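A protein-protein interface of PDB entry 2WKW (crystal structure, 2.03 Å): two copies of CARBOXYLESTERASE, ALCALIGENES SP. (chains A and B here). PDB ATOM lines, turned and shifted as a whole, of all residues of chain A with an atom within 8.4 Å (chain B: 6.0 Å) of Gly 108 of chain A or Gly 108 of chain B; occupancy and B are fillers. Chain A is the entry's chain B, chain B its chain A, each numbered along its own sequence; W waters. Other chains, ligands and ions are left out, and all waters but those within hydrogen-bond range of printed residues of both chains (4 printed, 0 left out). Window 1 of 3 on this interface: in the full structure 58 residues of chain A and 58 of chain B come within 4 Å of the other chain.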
ATOM      1  N   PHE A  22      -8.196  29.931   6.982  1.00  0.00           N
ATOM      2  CA  PHE A  22      -9.453  29.513   6.365  1.00  0.00           C
ATOM      3  C   PHE A  22     -10.454  30.646   6.477  1.00  0.00           C
ATOM      4  O   PHE A  22     -10.363  31.470   7.378  1.00  0.00           O
ATOM      5  CB  PHE A  22     -10.015  28.245   7.032  1.00  0.00           C
ATOM      6  CG  PHE A  22      -9.225  26.989   6.704  1.00  0.00           C
ATOM      7  CD1 PHE A  22      -8.053  26.701   7.387  1.00  0.00           C
ATOM      8  CD2 PHE A  22      -9.648  26.127   5.708  1.00  0.00           C
ATOM      9  CE1 PHE A  22      -7.291  25.572   7.077  1.00  0.00           C
ATOM     10  CE2 PHE A  22      -8.896  24.958   5.383  1.00  0.00           C
ATOM     11  CZ  PHE A  22      -7.720  24.689   6.083  1.00  0.00           C
ATOM     12  N   GLN A  49     -15.732  25.603   4.871  1.00  0.00           N
ATOM     13  CA  GLN A  49     -14.626  26.573   5.020  1.00  0.00           C
ATOM     14  C   GLN A  49     -13.681  26.521   3.804  1.00  0.00           C
ATOM     15  O   GLN A  49     -13.538  25.459   3.136  1.00  0.00           O
ATOM     16  CB  GLN A  49     -13.836  26.344   6.328  1.00  0.00           C
ATOM     17  CG  GLN A  49     -13.121  24.961   6.427  1.00  0.00           C
ATOM     18  CD  GLN A  49     -14.028  23.873   7.004  1.00  0.00           C
ATOM     19  OE1 GLN A  49     -15.232  23.905   6.792  1.00  0.00           O
ATOM     20  NE2 GLN A  49     -13.449  22.903   7.725  1.00  0.00           N
ATOM     21  N   TYR A  51      -9.825  27.023   2.376  1.00  0.00           N
ATOM     22  CA  TYR A  51      -8.373  27.134   2.547  1.00  0.00           C
ATOM     23  C   TYR A  51      -7.792  28.245   1.678  1.00  0.00           C
ATOM     24  O   TYR A  51      -8.077  28.302   0.482  1.00  0.00           O
ATOM     25  CB  TYR A  51      -7.698  25.826   2.110  1.00  0.00           C
ATOM     26  CG  TYR A  51      -6.181  25.840   2.158  1.00  0.00           C
ATOM     27  CD1 TYR A  51      -5.501  25.818   3.372  1.00  0.00           C
ATOM     28  CD2 TYR A  51      -5.426  25.816   0.979  1.00  0.00           C
ATOM     29  CE1 TYR A  51      -4.088  25.804   3.409  1.00  0.00           C
ATOM     30  CE2 TYR A  51      -4.025  25.794   1.012  1.00  0.00           C
ATOM     31  CZ  TYR A  51      -3.372  25.792   2.223  1.00  0.00           C
ATOM     32  OH  TYR A  51      -1.996  25.744   2.244  1.00  0.00           O
ATOM     33  N   HIS A  69      -9.150  28.210  -8.704  1.00  0.00           N
ATOM     34  CA  HIS A  69      -9.120  27.095  -9.661  1.00  0.00           C
ATOM     35  C   HIS A  69     -10.540  26.666 -10.099  1.00  0.00           C
ATOM     36  O   HIS A  69     -11.529  27.057  -9.478  1.00  0.00           O
ATOM     37  CB  HIS A  69      -8.399  25.899  -9.040  1.00  0.00           C
ATOM     38  CG  HIS A  69      -9.114  25.330  -7.862  1.00  0.00           C
ATOM     39  ND1 HIS A  69     -10.240  24.540  -7.986  1.00  0.00           N
ATOM     40  CD2 HIS A  69      -8.901  25.483  -6.530  1.00  0.00           C
ATOM     41  CE1 HIS A  69     -10.685  24.224  -6.779  1.00  0.00           C
ATOM     42  NE2 HIS A  69      -9.883  24.777  -5.880  1.00  0.00           N
ATOM     43  N   LEU A  73      -9.652  19.903  -9.886  1.00  0.00           N
ATOM     44  CA  LEU A  73      -8.305  20.437  -9.663  1.00  0.00           C
ATOM     45  C   LEU A  73      -8.312  21.170  -8.329  1.00  0.00           C
ATOM     46  O   LEU A  73      -9.381  21.382  -7.744  1.00  0.00           O
ATOM     47  CB  LEU A  73      -7.940  21.444 -10.786  1.00  0.00           C
ATOM     48  CG  LEU A  73      -7.839  20.936 -12.226  1.00  0.00           C
ATOM     49  CD1 LEU A  73      -7.929  22.090 -13.220  1.00  0.00           C
ATOM     50  CD2 LEU A  73      -6.501  20.120 -12.412  1.00  0.00           C
ATOM     51  N   THR A  74      -7.133  21.599  -7.878  1.00  0.00           N
ATOM     52  CA  THR A  74      -6.999  22.351  -6.630  1.00  0.00           C
ATOM     53  C   THR A  74      -6.164  23.613  -6.911  1.00  0.00           C
ATOM     54  O   THR A  74      -5.863  23.901  -8.060  1.00  0.00           O
ATOM     55  CB  THR A  74      -6.310  21.485  -5.507  1.00  0.00           C
ATOM     56  OG1 THR A  74      -4.939  21.262  -5.844  1.00  0.00           O
ATOM     57  CG2 THR A  74      -7.020  20.139  -5.294  1.00  0.00           C
ATOM     58  N   GLY A  75      -5.790  24.354  -5.870  1.00  0.00           N
ATOM     59  CA  GLY A  75      -4.828  25.475  -5.996  1.00  0.00           C
ATOM     60  C   GLY A  75      -3.479  25.092  -6.641  1.00  0.00           C
ATOM     61  O   GLY A  75      -2.735  25.955  -7.110  1.00  0.00           O
ATOM     62  N   MET A  76      -3.152  23.800  -6.649  1.00  0.00           N
ATOM     63  CA  MET A  76      -2.006  23.289  -7.417  1.00  0.00           C
ATOM     64  C   MET A  76      -2.008  23.808  -8.873  1.00  0.00           C
ATOM     65  O   MET A  76      -0.942  23.943  -9.499  1.00  0.00           O
ATOM     66  CB  MET A  76      -2.029  21.752  -7.419  1.00  0.00           C
ATOM     67  CG  MET A  76      -0.978  21.085  -8.349  1.00  0.00           C
ATOM     68  SD  MET A  76       0.706  21.369  -7.775  1.00  0.00           S
ATOM     69  CE  MET A  76       1.652  20.603  -9.135  1.00  0.00           C
ATOM     70  N   ILE A 102      -6.449  29.777  -3.323  1.00  0.00           N
ATOM     71  CA  ILE A 102      -7.423  29.022  -2.551  1.00  0.00           C
ATOM     72  C   ILE A 102      -7.551  27.562  -2.995  1.00  0.00           C
ATOM     73  O   ILE A 102      -7.157  27.202  -4.099  1.00  0.00           O
ATOM     74  CB  ILE A 102      -8.836  29.668  -2.609  1.00  0.00           C
ATOM     75  CG1 ILE A 102      -9.404  29.560  -4.031  1.00  0.00           C
ATOM     76  CG2 ILE A 102      -8.781  31.131  -2.130  1.00  0.00           C
ATOM     77  CD1 ILE A 102     -10.862  29.161  -4.115  1.00  0.00           C
ATOM     78  N   ASP A 103      -8.098  26.737  -2.100  1.00  0.00           N
ATOM     79  CA  ASP A 103      -8.802  25.540  -2.495  1.00  0.00           C
ATOM     80  C   ASP A 103     -10.277  25.860  -2.263  1.00  0.00           C
ATOM     81  O   ASP A 103     -10.656  26.273  -1.169  1.00  0.00           O
ATOM     82  CB  ASP A 103      -8.374  24.313  -1.654  1.00  0.00           C
ATOM     83  CG  ASP A 103      -7.056  23.719  -2.113  1.00  0.00           C
ATOM     84  OD1 ASP A 103      -6.573  24.143  -3.195  1.00  0.00           O
ATOM     85  OD2 ASP A 103      -6.511  22.816  -1.403  1.00  0.00           O
ATOM     86  N   GLN A 104     -11.094  25.674  -3.295  1.00  0.00           N
ATOM     87  CA  GLN A 104     -12.553  25.845  -3.189  1.00  0.00           C
ATOM     88  C   GLN A 104     -13.113  25.067  -1.995  1.00  0.00           C
ATOM     89  O   GLN A 104     -12.597  23.999  -1.659  1.00  0.00           O
ATOM     90  CB  GLN A 104     -13.232  25.293  -4.445  1.00  0.00           C
ATOM     91  CG  GLN A 104     -13.129  26.162  -5.699  1.00  0.00           C
ATOM     92  CD  GLN A 104     -14.111  25.692  -6.777  1.00  0.00           C
ATOM     93  OE1 GLN A 104     -15.248  25.341  -6.474  1.00  0.00           O
ATOM     94  NE2 GLN A 104     -13.658  25.660  -8.034  1.00  0.00           N
ATOM     95  N   SER A 105     -14.177  25.579  -1.374  1.00  0.00           N
ATOM     96  CA  SER A 105     -14.973  24.777  -0.438  1.00  0.00           C
ATOM     97  C   SER A 105     -15.153  23.355  -0.980  1.00  0.00           C
ATOM     98  O   SER A 105     -15.493  23.150  -2.157  1.00  0.00           O
ATOM     99  CB  SER A 105     -16.349  25.433  -0.231  1.00  0.00           C
ATOM    100  OG  SER A 105     -16.215  26.699   0.424  1.00  0.00           O
ATOM    101  N   GLY A 106     -14.946  22.362  -0.134  1.00  0.00           N
ATOM    102  CA  GLY A 106     -15.217  20.989  -0.539  1.00  0.00           C
ATOM    103  C   GLY A 106     -14.197  20.424  -1.530  1.00  0.00           C
ATOM    104  O   GLY A 106     -14.463  19.415  -2.185  1.00  0.00           O
ATOM    105  N   ARG A 107     -13.031  21.056  -1.631  1.00  0.00           N
ATOM    106  CA  ARG A 107     -11.974  20.579  -2.538  1.00  0.00           C
ATOM    107  C   ARG A 107     -10.616  20.687  -1.848  1.00  0.00           C
ATOM    108  O   ARG A 107     -10.414  21.584  -1.045  1.00  0.00           O
ATOM    109  CB  ARG A 107     -11.960  21.426  -3.831  1.00  0.00           C
ATOM    110  CG  ARG A 107     -11.157  20.807  -5.012  1.00  0.00           C
ATOM    111  CD  ARG A 107     -12.061  19.845  -5.870  1.00  0.00           C
ATOM    112  NE  ARG A 107     -13.301  20.529  -6.279  1.00  0.00           N
ATOM    113  CZ  ARG A 107     -13.385  21.427  -7.271  1.00  0.00           C
ATOM    114  NH1 ARG A 107     -12.309  21.732  -7.998  1.00  0.00           N
ATOM    115  NH2 ARG A 107     -14.550  22.012  -7.549  1.00  0.00           N
ATOM    116  N   GLY A 108      -9.674  19.799  -2.183  1.00  0.00           N
ATOM    117  CA  GLY A 108      -8.314  19.929  -1.652  1.00  0.00           C
ATOM    118  C   GLY A 108      -8.280  19.962  -0.131  1.00  0.00           C
ATOM    119  O   GLY A 108      -8.809  19.067   0.527  1.00  0.00           O
ATOM    120  N   ARG A 109      -7.683  21.012   0.431  1.00  0.00           N
ATOM    121  CA  ARG A 109      -7.531  21.106   1.889  1.00  0.00           C
ATOM    122  C   ARG A 109      -8.768  21.690   2.583  1.00  0.00           C
ATOM    123  O   ARG A 109      -8.771  21.865   3.816  1.00  0.00           O
ATOM    124  CB  ARG A 109      -6.276  21.906   2.219  1.00  0.00           C
ATOM    125  CG  ARG A 109      -4.987  21.223   1.668  1.00  0.00           C
ATOM    126  CD  ARG A 109      -3.732  21.997   1.959  1.00  0.00           C
ATOM    127  NE  ARG A 109      -2.533  21.154   1.843  1.00  0.00           N
ATOM    128  CZ  ARG A 109      -1.282  21.572   2.046  1.00  0.00           C
ATOM    129  NH1 ARG A 109      -1.017  22.856   2.295  1.00  0.00           N
ATOM    130  NH2 ARG A 109      -0.278  20.701   1.956  1.00  0.00           N
ATOM    131  N   SER A 110      -9.802  21.988   1.790  1.00  0.00           N
ATOM    132  CA  SER A 110     -11.098  22.508   2.317  1.00  0.00           C
ATOM    133  C   SER A 110     -12.069  21.343   2.555  1.00  0.00           C
ATOM    134  O   SER A 110     -12.425  20.619   1.617  1.00  0.00           O
ATOM    135  CB  SER A 110     -11.703  23.486   1.306  1.00  0.00           C
ATOM    136  OG  SER A 110     -10.789  24.542   1.056  1.00  0.00           O
ATOM    137  N   ALA A 111     -12.465  21.151   3.814  1.00  0.00           N
ATOM    138  CA  ALA A 111     -13.176  19.953   4.247  1.00  0.00           C
ATOM    139  C   ALA A 111     -14.522  19.718   3.550  1.00  0.00           C
ATOM    140  O   ALA A 111     -15.340  20.645   3.421  1.00  0.00           O
ATOM    141  CB  ALA A 111     -13.389  19.993   5.770  1.00  0.00           C
ATOM    142  N   THR A 112     -14.742  18.469   3.133  1.00  0.00           N
ATOM    143  CA  THR A 112     -16.075  17.975   2.726  1.00  0.00           C
ATOM    144  C   THR A 112     -16.773  17.443   3.986  1.00  0.00           C
ATOM    145  O   THR A 112     -16.168  17.395   5.069  1.00  0.00           O
ATOM    146  CB  THR A 112     -15.957  16.826   1.688  1.00  0.00           C
ATOM    147  OG1 THR A 112     -15.146  15.769   2.233  1.00  0.00           O
ATOM    148  CG2 THR A 112     -15.304  17.329   0.359  1.00  0.00           C
ATOM    149  N   GLN A 171      -2.472  15.755 -10.777  1.00  0.00           N
ATOM    150  CA  GLN A 171      -3.062  16.884  -9.985  1.00  0.00           C
ATOM    151  C   GLN A 171      -4.584  16.991 -10.049  1.00  0.00           C
ATOM    152  O   GLN A 171      -5.185  17.873  -9.405  1.00  0.00           O
ATOM    153  CB  GLN A 171      -2.404  18.236 -10.327  1.00  0.00           C
ATOM    154  CG  GLN A 171      -2.743  18.845 -11.695  1.00  0.00           C
ATOM    155  CD  GLN A 171      -2.154  20.252 -11.794  1.00  0.00           C
ATOM    156  OE1 GLN A 171      -0.954  20.425 -12.023  1.00  0.00           O
ATOM    157  NE2 GLN A 171      -2.976  21.248 -11.565  1.00  0.00           N
ATOM    158  N   VAL A 173      -8.406  15.764  -9.291  1.00  0.00           N
ATOM    159  CA  VAL A 173      -9.053  15.178  -8.116  1.00  0.00           C
ATOM    160  C   VAL A 173     -10.580  15.120  -8.301  1.00  0.00           C
ATOM    161  O   VAL A 173     -11.136  15.856  -9.136  1.00  0.00           O
ATOM    162  CB  VAL A 173      -8.742  16.023  -6.819  1.00  0.00           C
ATOM    163  CG1 VAL A 173      -7.216  16.056  -6.530  1.00  0.00           C
ATOM    164  CG2 VAL A 173      -9.315  17.455  -6.955  1.00  0.00           C
ATOM    165  N   PRO A 174     -11.260  14.263  -7.518  1.00  0.00           N
ATOM    166  CA  PRO A 174     -12.719  14.273  -7.467  1.00  0.00           C
ATOM    167  C   PRO A 174     -13.293  15.645  -7.110  1.00  0.00           C
ATOM    168  O   PRO A 174     -12.688  16.417  -6.340  1.00  0.00           O
ATOM    169  CB  PRO A 174     -13.027  13.282  -6.339  1.00  0.00           C
ATOM    170  CG  PRO A 174     -11.927  12.283  -6.423  1.00  0.00           C
ATOM    171  CD  PRO A 174     -10.700  13.113  -6.771  1.00  0.00           C
ATOM    172  N   ASP A 175     -14.472  15.912  -7.654  1.00  0.00           N
ATOM    173  CA  ASP A 175     -15.109  17.208  -7.536  1.00  0.00           C
ATOM    174  C   ASP A 175     -16.461  17.037  -6.852  1.00  0.00           C
ATOM    175  O   ASP A 175     -17.297  16.252  -7.307  1.00  0.00           O
ATOM    176  CB  ASP A 175     -15.280  17.802  -8.942  1.00  0.00           C
ATOM    177  CG  ASP A 175     -15.593  19.295  -8.917  1.00  0.00           C
ATOM    178  OD1 ASP A 175     -16.375  19.741  -8.047  1.00  0.00           O
ATOM    179  OD2 ASP A 175     -15.041  20.022  -9.762  1.00  0.00           O
ATOM    180  N   TRP A 176     -16.660  17.770  -5.757  1.00  0.00           N
ATOM    181  CA  TRP A 176     -17.882  17.685  -4.943  1.00  0.00           C
ATOM    182  C   TRP A 176     -18.904  18.809  -5.242  1.00  0.00           C
ATOM    183  O   TRP A 176     -19.930  18.929  -4.557  1.00  0.00           O
ATOM    184  CB  TRP A 176     -17.506  17.687  -3.452  1.00  0.00           C
ATOM    185  CG  TRP A 176     -16.927  16.382  -2.970  1.00  0.00           C
ATOM    186  CD1 TRP A 176     -15.849  15.715  -3.493  1.00  0.00           C
ATOM    187  CD2 TRP A 176     -17.390  15.587  -1.860  1.00  0.00           C
ATOM    188  NE1 TRP A 176     -15.627  14.552  -2.789  1.00  0.00           N
ATOM    189  CE2 TRP A 176     -16.549  14.454  -1.778  1.00  0.00           C
ATOM    190  CE3 TRP A 176     -18.442  15.720  -0.938  1.00  0.00           C
ATOM    191  CZ2 TRP A 176     -16.724  13.454  -0.805  1.00  0.00           C
ATOM    192  CZ3 TRP A 176     -18.611  14.739   0.038  1.00  0.00           C
ATOM    193  CH2 TRP A 176     -17.757  13.616   0.093  1.00  0.00           C
ATOM    194  N   LEU B  73      -6.413  15.643   9.012  1.00  0.00           N
ATOM    195  CA  LEU B  73      -5.668  16.889   8.778  1.00  0.00           C
ATOM    196  C   LEU B  73      -4.910  16.803   7.457  1.00  0.00           C
ATOM    197  O   LEU B  73      -4.813  15.719   6.844  1.00  0.00           O
ATOM    198  CB  LEU B  73      -4.632  17.129   9.908  1.00  0.00           C
ATOM    199  CG  LEU B  73      -5.125  17.310  11.353  1.00  0.00           C
ATOM    200  CD1 LEU B  73      -4.056  16.902  12.408  1.00  0.00           C
ATOM    201  CD2 LEU B  73      -5.675  18.720  11.576  1.00  0.00           C
ATOM    202  N   THR B  74      -4.306  17.922   7.056  1.00  0.00           N
ATOM    203  CA  THR B  74      -3.469  17.954   5.851  1.00  0.00           C
ATOM    204  C   THR B  74      -2.107  18.590   6.205  1.00  0.00           C
ATOM    205  O   THR B  74      -1.802  18.783   7.387  1.00  0.00           O
ATOM    206  CB  THR B  74      -4.156  18.734   4.692  1.00  0.00           C
ATOM    207  OG1 THR B  74      -4.234  20.119   5.041  1.00  0.00           O
ATOM    208  CG2 THR B  74      -5.576  18.211   4.383  1.00  0.00           C
ATOM    209  N   ASP B 103       0.695  16.349   1.307  1.00  0.00           N
ATOM    210  CA  ASP B 103      -0.598  15.767   1.667  1.00  0.00           C
ATOM    211  C   ASP B 103      -0.502  14.255   1.449  1.00  0.00           C
ATOM    212  O   ASP B 103      -0.121  13.817   0.350  1.00  0.00           O
ATOM    213  CB  ASP B 103      -1.724  16.374   0.823  1.00  0.00           C
ATOM    214  CG  ASP B 103      -2.095  17.777   1.298  1.00  0.00           C
ATOM    215  OD1 ASP B 103      -1.607  18.151   2.384  1.00  0.00           O
ATOM    216  OD2 ASP B 103      -2.858  18.494   0.605  1.00  0.00           O
ATOM    217  N   GLN B 104      -0.837  13.453   2.470  1.00  0.00           N
ATOM    218  CA  GLN B 104      -0.825  11.968   2.307  1.00  0.00           C
ATOM    219  C   GLN B 104      -1.633  11.569   1.073  1.00  0.00           C
ATOM    220  O   GLN B 104      -2.580  12.281   0.702  1.00  0.00           O
ATOM    221  CB  GLN B 104      -1.481  11.271   3.493  1.00  0.00           C
ATOM    222  CG  GLN B 104      -0.702  11.270   4.784  1.00  0.00           C
ATOM    223  CD  GLN B 104      -1.355  10.350   5.830  1.00  0.00           C
ATOM    224  OE1 GLN B 104      -1.872   9.271   5.502  1.00  0.00           O
ATOM    225  NE2 GLN B 104      -1.357  10.784   7.075  1.00  0.00           N
ATOM    226  N   GLY B 106      -4.542  10.146  -0.827  1.00  0.00           N
ATOM    227  CA  GLY B 106      -5.960  10.123  -0.441  1.00  0.00           C
ATOM    228  C   GLY B 106      -6.407  11.198   0.535  1.00  0.00           C
ATOM    229  O   GLY B 106      -7.478  11.077   1.152  1.00  0.00           O
ATOM    230  N   ARG B 107      -5.610  12.254   0.677  1.00  0.00           N
ATOM    231  CA  ARG B 107      -5.979  13.368   1.576  1.00  0.00           C
ATOM    232  C   ARG B 107      -5.656  14.711   0.947  1.00  0.00           C
ATOM    233  O   ARG B 107      -4.710  14.821   0.189  1.00  0.00           O
ATOM    234  CB  ARG B 107      -5.225  13.262   2.920  1.00  0.00           C
ATOM    235  CG  ARG B 107      -5.812  14.175   4.062  1.00  0.00           C
ATOM    236  CD  ARG B 107      -6.853  13.405   4.890  1.00  0.00           C
ATOM    237  NE  ARG B 107      -6.347  12.082   5.278  1.00  0.00           N
ATOM    238  CZ  ARG B 107      -5.477  11.851   6.257  1.00  0.00           C
ATOM    239  NH1 ARG B 107      -5.021  12.847   6.999  1.00  0.00           N
ATOM    240  NH2 ARG B 107      -5.047  10.605   6.495  1.00  0.00           N
ATOM    241  N   GLY B 108      -6.412  15.759   1.268  1.00  0.00           N
ATOM    242  CA  GLY B 108      -6.064  17.080   0.734  1.00  0.00           C
ATOM    243  C   GLY B 108      -6.009  17.139  -0.791  1.00  0.00           C
ATOM    244  O   GLY B 108      -6.953  16.731  -1.478  1.00  0.00           O
ATOM    245  N   ARG B 109      -4.879  17.621  -1.311  1.00  0.00           N
ATOM    246  CA  ARG B 109      -4.677  17.792  -2.743  1.00  0.00           C
ATOM    247  C   ARG B 109      -4.275  16.488  -3.466  1.00  0.00           C
ATOM    248  O   ARG B 109      -4.081  16.481  -4.692  1.00  0.00           O
ATOM    249  CB  ARG B 109      -3.642  18.905  -2.993  1.00  0.00           C
ATOM    250  CG  ARG B 109      -4.188  20.290  -2.538  1.00  0.00           C
ATOM    251  CD  ARG B 109      -3.119  21.377  -2.550  1.00  0.00           C
ATOM    252  NE  ARG B 109      -3.757  22.681  -2.515  1.00  0.00           N
ATOM    253  CZ  ARG B 109      -3.145  23.846  -2.687  1.00  0.00           C
ATOM    254  NH1 ARG B 109      -1.823  23.920  -2.884  1.00  0.00           N
ATOM    255  NH2 ARG B 109      -3.878  24.952  -2.663  1.00  0.00           N
ATOM    256  N   SER B 110      -4.177  15.402  -2.701  1.00  0.00           N
ATOM    257  CA  SER B 110      -3.851  14.066  -3.252  1.00  0.00           C
ATOM    258  C   SER B 110      -5.151  13.268  -3.497  1.00  0.00           C
ATOM    259  O   SER B 110      -5.931  12.995  -2.538  1.00  0.00           O
ATOM    260  CB  SER B 110      -2.938  13.292  -2.278  1.00  0.00           C
ATOM    261  OG  SER B 110      -1.763  14.021  -1.928  1.00  0.00           O
ATOM    262  N   ALA B 111      -5.388  12.914  -4.768  1.00  0.00           N
ATOM    263  CA  ALA B 111      -6.699  12.360  -5.232  1.00  0.00           C
ATOM    264  C   ALA B 111      -7.144  11.063  -4.565  1.00  0.00           C
ATOM    265  O   ALA B 111      -6.366  10.107  -4.458  1.00  0.00           O
ATOM    266  CB  ALA B 111      -6.705  12.133  -6.760  1.00  0.00           C
ATOM    267  N   VAL B 173     -10.298  17.623   8.337  1.00  0.00           N
ATOM    268  CA  VAL B 173     -10.915  17.123   7.117  1.00  0.00           C
ATOM    269  C   VAL B 173     -11.219  15.610   7.254  1.00  0.00           C
ATOM    270  O   VAL B 173     -10.651  14.923   8.119  1.00  0.00           O
ATOM    271  CB  VAL B 173      -9.991  17.338   5.876  1.00  0.00           C
ATOM    272  CG1 VAL B 173      -9.643  18.827   5.689  1.00  0.00           C
ATOM    273  CG2 VAL B 173      -8.709  16.471   5.995  1.00  0.00           C
HETATM  274  O   HOH W   1      -8.973  17.395  -3.576  1.00  0.00           O
HETATM  275  O   HOH W   2      -6.681  21.197   5.833  1.00  0.00           O
HETATM  276  O   HOH W   3      -4.304  18.666  -6.785  1.00  0.00           O
HETATM  277  O   HOH W   4      -8.590  16.942   2.565  1.00  0.00           O
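Printed residues of chain A that touch a printed residue of chain B: Tyr 51, Thr 74, Gly 75, Met 76, Asp 103, Gly 108, Arg 109, Ala 111 and Val 173.
Hydrophobic or aromatic side chains of chain A within 4 Å of the printed part of chain B: Tyr 51, Ala 111 and Val 173.
Hydrophobic or aromatic side chains of chain B that line the printed part of chain A: Ala 111 and Val 173.
Thr 74 of chain A touches Arg 109 of chain B, and with the chains exchanged Arg 109 of chain A touches Thr 74 of chain B.
Gly 108 of chain B touches its own counterpart, Gly 108 of chain A.
Arg 109 of chain A touches Val 173 of chain B, and with the chains exchanged Val 173 of chain A touches Arg 109 of chain B.
Ala 111 of chain A touches Val 173 of chain B, and with the chains exchanged Val 173 of chain A touches Ala 111 of chain B.
Positions printed for both chains: 73, 74, 103, 104, 106, 107, 108, 109, 110, 111 and 173.
Of the 12 pairs that touch across the chains among the printed residues, 9 have their exchanged pair printed and touching as well.
The backbone NH of Arg 109 of chain B is in hydrogen-bond range of the side-chain carboxylate of Asp 103 of chain B (2.9 Å).
The backbone carbonyl oxygen (O) of Asp 103 of chain B lies within hydrogen-bond range of the side-chain hydroxyl (OG) of Ser 110 of chain B (2.8 Å).
The side-chain hydroxyl of Ser 110 of chain A sits at hydrogen-bond distance from the backbone NH of Tyr 51 of chain A, at 3.0 Å.
N of Met 76 of chain A lies close to OG1 of Thr 74 of chain A.
OD2 of Asp 103 of chain A sits at hydrogen-bond distance from N of Arg 109 of chain A (2.8 Å).
The side-chain hydroxyl (OG) of Ser 110 of chain A sits at hydrogen-bond distance from the backbone carbonyl oxygen (O) of Asp 103 of chain A.
Arg 109 of chain B touches Tyr 51 of chain A.
Thr 74 of chain A touches Arg 109 of chain B.
Gly 75 of chain A touches Arg 109 of chain B.
Met 76 of chain A touches Arg 109 of chain B (N to CZ, 3.96 Å).
Gly 108 of chain B touches Gly 108 of chain A.
Thr 74 of chain B touches Arg 109 of chain A (OG1 to CG, 3.6 Å).
Arg 109 of chain A touches Val 173 of chain B.
CB of Ala 111 of chain A touches CG1 of Val 173 of chain B (3.9 Å).
CG1 of Val 173 of chain A touches O of Arg 109 of chain B (3.7 Å).
Ala 111 of chain B touches Val 173 of chain A.
The side-chain carboxylate (OD1) of Asp 103 of chain B lies within salt-bridge range of the guanidinium group (NH2) of Arg 109 of chain A (2.9 Å).
OD1 of Asp 103 of chain A is in salt-bridge range of NH2 of Arg 109 of chain B, at 2.9 Å.
Of chain B, only Gly 108 (3.4 Å) comes within 4 Å of Gly 108 of chain A.
Of chain A, only Gly 108 comes within 4 Å of Gly 108 of chain B.
Of the printed residues of chain B, Val 173 of chain A touches Arg 109 (3.7 Å) and Ala 111 (3.95 Å).
Of the printed residues of chain A, Arg 109 of chain B touches Tyr 51, Thr 74, Gly 75, Met 76, Asp 103 and Val 173.
His 69 of chain A touches none of the printed residues of chain B.
The nearest residue of chain A that does not touch Gly 108 of chain B is Arg 109 of chain A (4.3 Å).
The nearest printed residue of chain B that does not touch Val 173 of chain A is Ser 110 of chain B (4.6 Å).
Water W2 bridges OG1 of Thr 74 of chain B and O of Arg 109 of chain A.
Water W4 lies within hydrogen-bond range of the backbone NH (N) of Gly 108 of chain B (2.8 Å) and the backbone carbonyl oxygen (O) of Gly 108 of chain A (3.0 Å).
Water W3 lies within hydrogen-bond range of OG1 of Thr 74 of chain A (2.8 Å), O of Gln 171 of chain A (2.9 Å) and O of Arg 109 of chain B (3.0 Å).
Water W1 lies within hydrogen-bond range of the backbone NH (N) of Gly 108 of chain A and the backbone carbonyl oxygen (O) of Gly 108 of chain B.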
